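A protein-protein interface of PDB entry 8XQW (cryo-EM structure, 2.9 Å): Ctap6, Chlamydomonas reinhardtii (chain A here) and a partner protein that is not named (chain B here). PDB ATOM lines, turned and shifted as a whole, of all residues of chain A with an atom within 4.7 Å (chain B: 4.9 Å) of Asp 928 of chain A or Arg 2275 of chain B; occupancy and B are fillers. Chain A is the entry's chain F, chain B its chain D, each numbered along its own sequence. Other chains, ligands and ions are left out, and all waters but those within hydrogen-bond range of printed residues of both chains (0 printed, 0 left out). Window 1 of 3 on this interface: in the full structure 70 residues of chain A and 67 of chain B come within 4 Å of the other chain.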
ATOM      1  N   TYR A 926     -16.595 -15.672 -26.352  1.00  0.00           N
ATOM      2  CA  TYR A 926     -16.291 -14.694 -25.326  1.00  0.00           C
ATOM      3  C   TYR A 926     -17.548 -14.435 -24.526  1.00  0.00           C
ATOM      4  O   TYR A 926     -18.603 -14.172 -25.098  1.00  0.00           O
ATOM      5  CB  TYR A 926     -15.768 -13.390 -25.919  1.00  0.00           C
ATOM      6  CG  TYR A 926     -14.443 -13.563 -26.584  1.00  0.00           C
ATOM      7  CD1 TYR A 926     -13.273 -13.413 -25.877  1.00  0.00           C
ATOM      8  CD2 TYR A 926     -14.361 -13.912 -27.912  1.00  0.00           C
ATOM      9  CE1 TYR A 926     -12.068 -13.591 -26.471  1.00  0.00           C
ATOM     10  CE2 TYR A 926     -13.158 -14.091 -28.515  1.00  0.00           C
ATOM     11  CZ  TYR A 926     -12.012 -13.936 -27.791  1.00  0.00           C
ATOM     12  OH  TYR A 926     -10.798 -14.119 -28.397  1.00  0.00           O
ATOM     13  N   PHE A 927     -17.440 -14.512 -23.210  1.00  0.00           N
ATOM     14  CA  PHE A 927     -18.588 -14.381 -22.333  1.00  0.00           C
ATOM     15  C   PHE A 927     -18.584 -13.023 -21.661  1.00  0.00           C
ATOM     16  O   PHE A 927     -17.538 -12.395 -21.503  1.00  0.00           O
ATOM     17  CB  PHE A 927     -18.602 -15.474 -21.293  1.00  0.00           C
ATOM     18  CG  PHE A 927     -18.667 -16.826 -21.882  1.00  0.00           C
ATOM     19  CD1 PHE A 927     -17.525 -17.467 -22.274  1.00  0.00           C
ATOM     20  CD2 PHE A 927     -19.872 -17.439 -22.079  1.00  0.00           C
ATOM     21  CE1 PHE A 927     -17.585 -18.697 -22.834  1.00  0.00           C
ATOM     22  CE2 PHE A 927     -19.934 -18.669 -22.636  1.00  0.00           C
ATOM     23  CZ  PHE A 927     -18.790 -19.299 -23.016  1.00  0.00           C
ATOM     24  N   ASP A 928     -19.764 -12.573 -21.273  1.00  0.00           N
ATOM     25  CA  ASP A 928     -19.891 -11.276 -20.638  1.00  0.00           C
ATOM     26  C   ASP A 928     -20.952 -11.334 -19.553  1.00  0.00           C
ATOM     27  O   ASP A 928     -21.917 -12.092 -19.658  1.00  0.00           O
ATOM     28  CB  ASP A 928     -20.241 -10.206 -21.657  1.00  0.00           C
ATOM     29  CG  ASP A 928     -20.433  -8.857 -21.024  1.00  0.00           C
ATOM     30  OD1 ASP A 928     -19.539  -8.419 -20.273  1.00  0.00           O
ATOM     31  OD2 ASP A 928     -21.478  -8.231 -21.276  1.00  0.00           O
ATOM     32  N   GLY A 929     -20.767 -10.543 -18.505  1.00  0.00           N
ATOM     33  CA  GLY A 929     -21.713 -10.535 -17.411  1.00  0.00           C
ATOM     34  C   GLY A 929     -23.028  -9.880 -17.759  1.00  0.00           C
ATOM     35  O   GLY A 929     -23.054  -8.769 -18.297  1.00  0.00           O
ATOM     36  N   SER A 930     -24.128 -10.555 -17.456  1.00  0.00           N
ATOM     37  CA  SER A 930     -25.455 -10.009 -17.696  1.00  0.00           C
ATOM     38  C   SER A 930     -25.912  -9.214 -16.474  1.00  0.00           C
ATOM     39  O   SER A 930     -25.124  -8.899 -15.576  1.00  0.00           O
ATOM     40  CB  SER A 930     -26.434 -11.120 -18.050  1.00  0.00           C
ATOM     41  OG  SER A 930     -26.499 -11.303 -19.450  1.00  0.00           O
ATOM     42  N   ARG A 935     -25.582 -14.841 -14.496  1.00  0.00           N
ATOM     43  CA  ARG A 935     -25.957 -14.859 -15.899  1.00  0.00           C
ATOM     44  C   ARG A 935     -24.806 -14.380 -16.768  1.00  0.00           C
ATOM     45  O   ARG A 935     -24.247 -13.305 -16.542  1.00  0.00           O
ATOM     46  CB  ARG A 935     -27.182 -13.985 -16.139  1.00  0.00           C
ATOM     47  CG  ARG A 935     -28.370 -14.373 -15.306  1.00  0.00           C
ATOM     48  CD  ARG A 935     -29.457 -14.960 -16.163  1.00  0.00           C
ATOM     49  NE  ARG A 935     -29.828 -14.054 -17.236  1.00  0.00           N
ATOM     50  CZ  ARG A 935     -30.766 -14.324 -18.129  1.00  0.00           C
ATOM     51  NH1 ARG A 935     -31.423 -15.470 -18.069  1.00  0.00           N
ATOM     52  NH2 ARG A 935     -31.045 -13.447 -19.076  1.00  0.00           N
ATOM     53  N   PHE A 936     -24.469 -15.184 -17.773  1.00  0.00           N
ATOM     54  CA  PHE A 936     -23.430 -14.863 -18.737  1.00  0.00           C
ATOM     55  C   PHE A 936     -24.004 -14.939 -20.137  1.00  0.00           C
ATOM     56  O   PHE A 936     -24.779 -15.844 -20.449  1.00  0.00           O
ATOM     57  CB  PHE A 936     -22.256 -15.814 -18.622  1.00  0.00           C
ATOM     58  CG  PHE A 936     -21.471 -15.649 -17.368  1.00  0.00           C
ATOM     59  CD1 PHE A 936     -20.811 -14.472 -17.104  1.00  0.00           C
ATOM     60  CD2 PHE A 936     -21.389 -16.674 -16.453  1.00  0.00           C
ATOM     61  CE1 PHE A 936     -20.089 -14.318 -15.950  1.00  0.00           C
ATOM     62  CE2 PHE A 936     -20.669 -16.522 -15.300  1.00  0.00           C
ATOM     63  CZ  PHE A 936     -20.019 -15.344 -15.050  1.00  0.00           C
ATOM     64  N   GLN A 937     -23.617 -13.992 -20.978  1.00  0.00           N
ATOM     65  CA  GLN A 937     -24.011 -13.973 -22.376  1.00  0.00           C
ATOM     66  C   GLN A 937     -22.824 -14.344 -23.243  1.00  0.00           C
ATOM     67  O   GLN A 937     -21.723 -13.827 -23.055  1.00  0.00           O
ATOM     68  CB  GLN A 937     -24.528 -12.601 -22.782  1.00  0.00           C
ATOM     69  CG  GLN A 937     -25.085 -12.578 -24.169  1.00  0.00           C
ATOM     70  CD  GLN A 937     -25.766 -11.286 -24.489  1.00  0.00           C
ATOM     71  OE1 GLN A 937     -25.485 -10.262 -23.882  1.00  0.00           O
ATOM     72  NE2 GLN A 937     -26.676 -11.322 -25.443  1.00  0.00           N
ATOM     73  N   SER B2273     -16.347  -5.046 -17.796  1.00  0.00           N
ATOM     74  CA  SER B2273     -17.690  -5.326 -18.284  1.00  0.00           C
ATOM     75  C   SER B2273     -17.961  -4.492 -19.521  1.00  0.00           C
ATOM     76  O   SER B2273     -17.846  -3.265 -19.485  1.00  0.00           O
ATOM     77  CB  SER B2273     -18.731  -5.037 -17.210  1.00  0.00           C
ATOM     78  OG  SER B2273     -19.168  -3.702 -17.305  1.00  0.00           O
ATOM     79  N   VAL B2274     -18.340  -5.163 -20.609  1.00  0.00           N
ATOM     80  CA  VAL B2274     -18.629  -4.478 -21.859  1.00  0.00           C
ATOM     81  C   VAL B2274     -19.845  -3.578 -21.719  1.00  0.00           C
ATOM     82  O   VAL B2274     -19.869  -2.455 -22.238  1.00  0.00           O
ATOM     83  CB  VAL B2274     -18.826  -5.512 -22.976  1.00  0.00           C
ATOM     84  CG1 VAL B2274     -19.232  -4.832 -24.242  1.00  0.00           C
ATOM     85  CG2 VAL B2274     -17.561  -6.292 -23.183  1.00  0.00           C
ATOM     86  N   ARG B2275     -20.873  -4.054 -21.023  1.00  0.00           N
ATOM     87  CA  ARG B2275     -22.114  -3.305 -20.909  1.00  0.00           C
ATOM     88  C   ARG B2275     -21.871  -1.928 -20.306  1.00  0.00           C
ATOM     89  O   ARG B2275     -22.346  -0.915 -20.831  1.00  0.00           O
ATOM     90  CB  ARG B2275     -23.108  -4.099 -20.069  1.00  0.00           C
ATOM     91  CG  ARG B2275     -24.553  -3.776 -20.356  1.00  0.00           C
ATOM     92  CD  ARG B2275     -25.488  -4.778 -19.696  1.00  0.00           C
ATOM     93  NE  ARG B2275     -25.880  -5.853 -20.603  1.00  0.00           N
ATOM     94  CZ  ARG B2275     -25.285  -7.038 -20.653  1.00  0.00           C
ATOM     95  NH1 ARG B2275     -24.271  -7.304 -19.847  1.00  0.00           N
ATOM     96  NH2 ARG B2275     -25.705  -7.958 -21.508  1.00  0.00           N
ATOM     97  N   ALA B2276     -21.103  -1.869 -19.219  1.00  0.00           N
ATOM     98  CA  ALA B2276     -20.888  -0.601 -18.535  1.00  0.00           C
ATOM     99  C   ALA B2276     -20.064   0.355 -19.377  1.00  0.00           C
ATOM    100  O   ALA B2276     -20.380   1.548 -19.463  1.00  0.00           O
ATOM    101  CB  ALA B2276     -20.211  -0.837 -17.194  1.00  0.00           C
ATOM    102  N   LYS B2277     -19.005  -0.147 -20.011  1.00  0.00           N
ATOM    103  CA  LYS B2277     -18.157   0.709 -20.830  1.00  0.00           C
ATOM    104  C   LYS B2277     -18.928   1.287 -22.003  1.00  0.00           C
ATOM    105  O   LYS B2277     -18.833   2.484 -22.302  1.00  0.00           O
ATOM    106  CB  LYS B2277     -16.956  -0.077 -21.336  1.00  0.00           C
ATOM    107  CG  LYS B2277     -16.115   0.711 -22.295  1.00  0.00           C
ATOM    108  CD  LYS B2277     -15.029  -0.131 -22.890  1.00  0.00           C
ATOM    109  CE  LYS B2277     -14.114   0.719 -23.730  1.00  0.00           C
ATOM    110  NZ  LYS B2277     -13.250  -0.118 -24.597  1.00  0.00           N
ATOM    111  N   VAL B2278     -19.700   0.447 -22.683  1.00  0.00           N
ATOM    112  CA  VAL B2278     -20.447   0.917 -23.839  1.00  0.00           C
ATOM    113  C   VAL B2278     -21.525   1.901 -23.414  1.00  0.00           C
ATOM    114  O   VAL B2278     -21.765   2.906 -24.091  1.00  0.00           O
ATOM    115  CB  VAL B2278     -21.025  -0.276 -24.605  1.00  0.00           C
ATOM    116  CG1 VAL B2278     -21.963   0.202 -25.654  1.00  0.00           C
ATOM    117  CG2 VAL B2278     -19.911  -1.054 -25.228  1.00  0.00           C
ATOM    118  N   ALA B2279     -22.184   1.646 -22.282  1.00  0.00           N
ATOM    119  CA  ALA B2279     -23.181   2.589 -21.794  1.00  0.00           C
ATOM    120  C   ALA B2279     -22.555   3.938 -21.482  1.00  0.00           C
ATOM    121  O   ALA B2279     -23.133   4.984 -21.790  1.00  0.00           O
ATOM    122  CB  ALA B2279     -23.872   2.022 -20.560  1.00  0.00           C
ATOM    123  N   LYS B2705     -21.460  -3.361 -28.546  1.00  0.00           N
ATOM    124  CA  LYS B2705     -21.245  -4.513 -27.686  1.00  0.00           C
ATOM    125  C   LYS B2705     -20.580  -5.646 -28.441  1.00  0.00           C
ATOM    126  O   LYS B2705     -19.844  -6.440 -27.851  1.00  0.00           O
ATOM    127  CB  LYS B2705     -22.569  -4.990 -27.109  1.00  0.00           C
ATOM    128  CG  LYS B2705     -22.988  -4.300 -25.849  1.00  0.00           C
ATOM    129  CD  LYS B2705     -24.251  -4.927 -25.334  1.00  0.00           C
ATOM    130  CE  LYS B2705     -25.035  -3.949 -24.505  1.00  0.00           C
ATOM    131  NZ  LYS B2705     -26.383  -4.482 -24.184  1.00  0.00           N
ATOM    132  N   ARG B2712     -11.357  -7.841 -28.416  1.00  0.00           N
ATOM    133  CA  ARG B2712     -10.766  -8.879 -27.579  1.00  0.00           C
ATOM    134  C   ARG B2712     -10.138  -9.973 -28.422  1.00  0.00           C
ATOM    135  O   ARG B2712      -9.029 -10.433 -28.142  1.00  0.00           O
ATOM    136  CB  ARG B2712     -11.810  -9.499 -26.669  1.00  0.00           C
ATOM    137  CG  ARG B2712     -12.245  -8.674 -25.516  1.00  0.00           C
ATOM    138  CD  ARG B2712     -13.090  -9.553 -24.658  1.00  0.00           C
ATOM    139  NE  ARG B2712     -13.908  -8.824 -23.715  1.00  0.00           N
ATOM    140  CZ  ARG B2712     -14.849  -9.401 -22.988  1.00  0.00           C
ATOM    141  NH1 ARG B2712     -15.064 -10.695 -23.110  1.00  0.00           N
ATOM    142  NH2 ARG B2712     -15.570  -8.694 -22.142  1.00  0.00           N
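The side-chain carboxylate of Asp 928 of chain A sits at hydrogen-bond distance from the backbone NH of Val 2274 of chain B (3.5 Å). The guanidinium group of Arg 2275 of chain B lies within salt-bridge range of the side-chain carboxylate of Asp 928 of chain A (3.3 Å). The guanidinium group (NH1) of Arg 2275 of chain B lies within hydrogen-bond range of the backbone carbonyl oxygen (O) of Gly 929 of chain A. The guanidinium group (NH2) of Arg 2275 of chain B sits at hydrogen-bond distance from the side-chain amide oxygen (OE1) of Gln 937 of chain A, at 3.3 Å. O of Phe 927 of chain A is in hydrogen-bond range of NH1 of Arg 2712 of chain B (3.4 Å).
N of Gln 937 of chain A lies within hydrogen-bond range of O of Asp 928 of chain A (2.9 Å). The backbone NH (N) of Ser 930 of chain A is in hydrogen-bond range of the backbone carbonyl oxygen (O) of Arg 935 of chain A (2.9 Å).
Among the printed residues, pairs that only touch across the chains: Tyr 926 of chain A with Arg 2712 of chain B (3.96 Å) and Ser 930 of chain A with Arg 2275 of chain B (3.7 Å).
Arg 2275 of chain B touches just these residues of chain A: Asp 928 (3.3 Å), Gly 929 (2.5 Å), Ser 930 (3.7 Å) and Gln 937 (3.3 Å). Printed residues of chain B within 4 Å of Phe 927 of chain A: Arg 2712 (3.4 Å). Printed residues of chain B within 4 Å of Gly 929 of chain A: Arg 2275. Of the printed residues of chain B, Ser 930 of chain A touches Arg 2275. Ala 2276 of chain B touches none of the printed residues of chain A. Lys 2705 of chain B touches none of the printed residues of chain A. The nearest residue of chain B that does not touch Asp 928 of chain A is Ser 2273 of chain B (4.1 Å).
Of the 9 printed residues of chain B, 3 touch a printed residue of chain A. Among the printed residues, Asp or Glu carboxylates within 4 Å of a Lys or Arg side-chain nitrogen of the other chain: Asp 928 of chain A with Arg 2275 of chain B.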
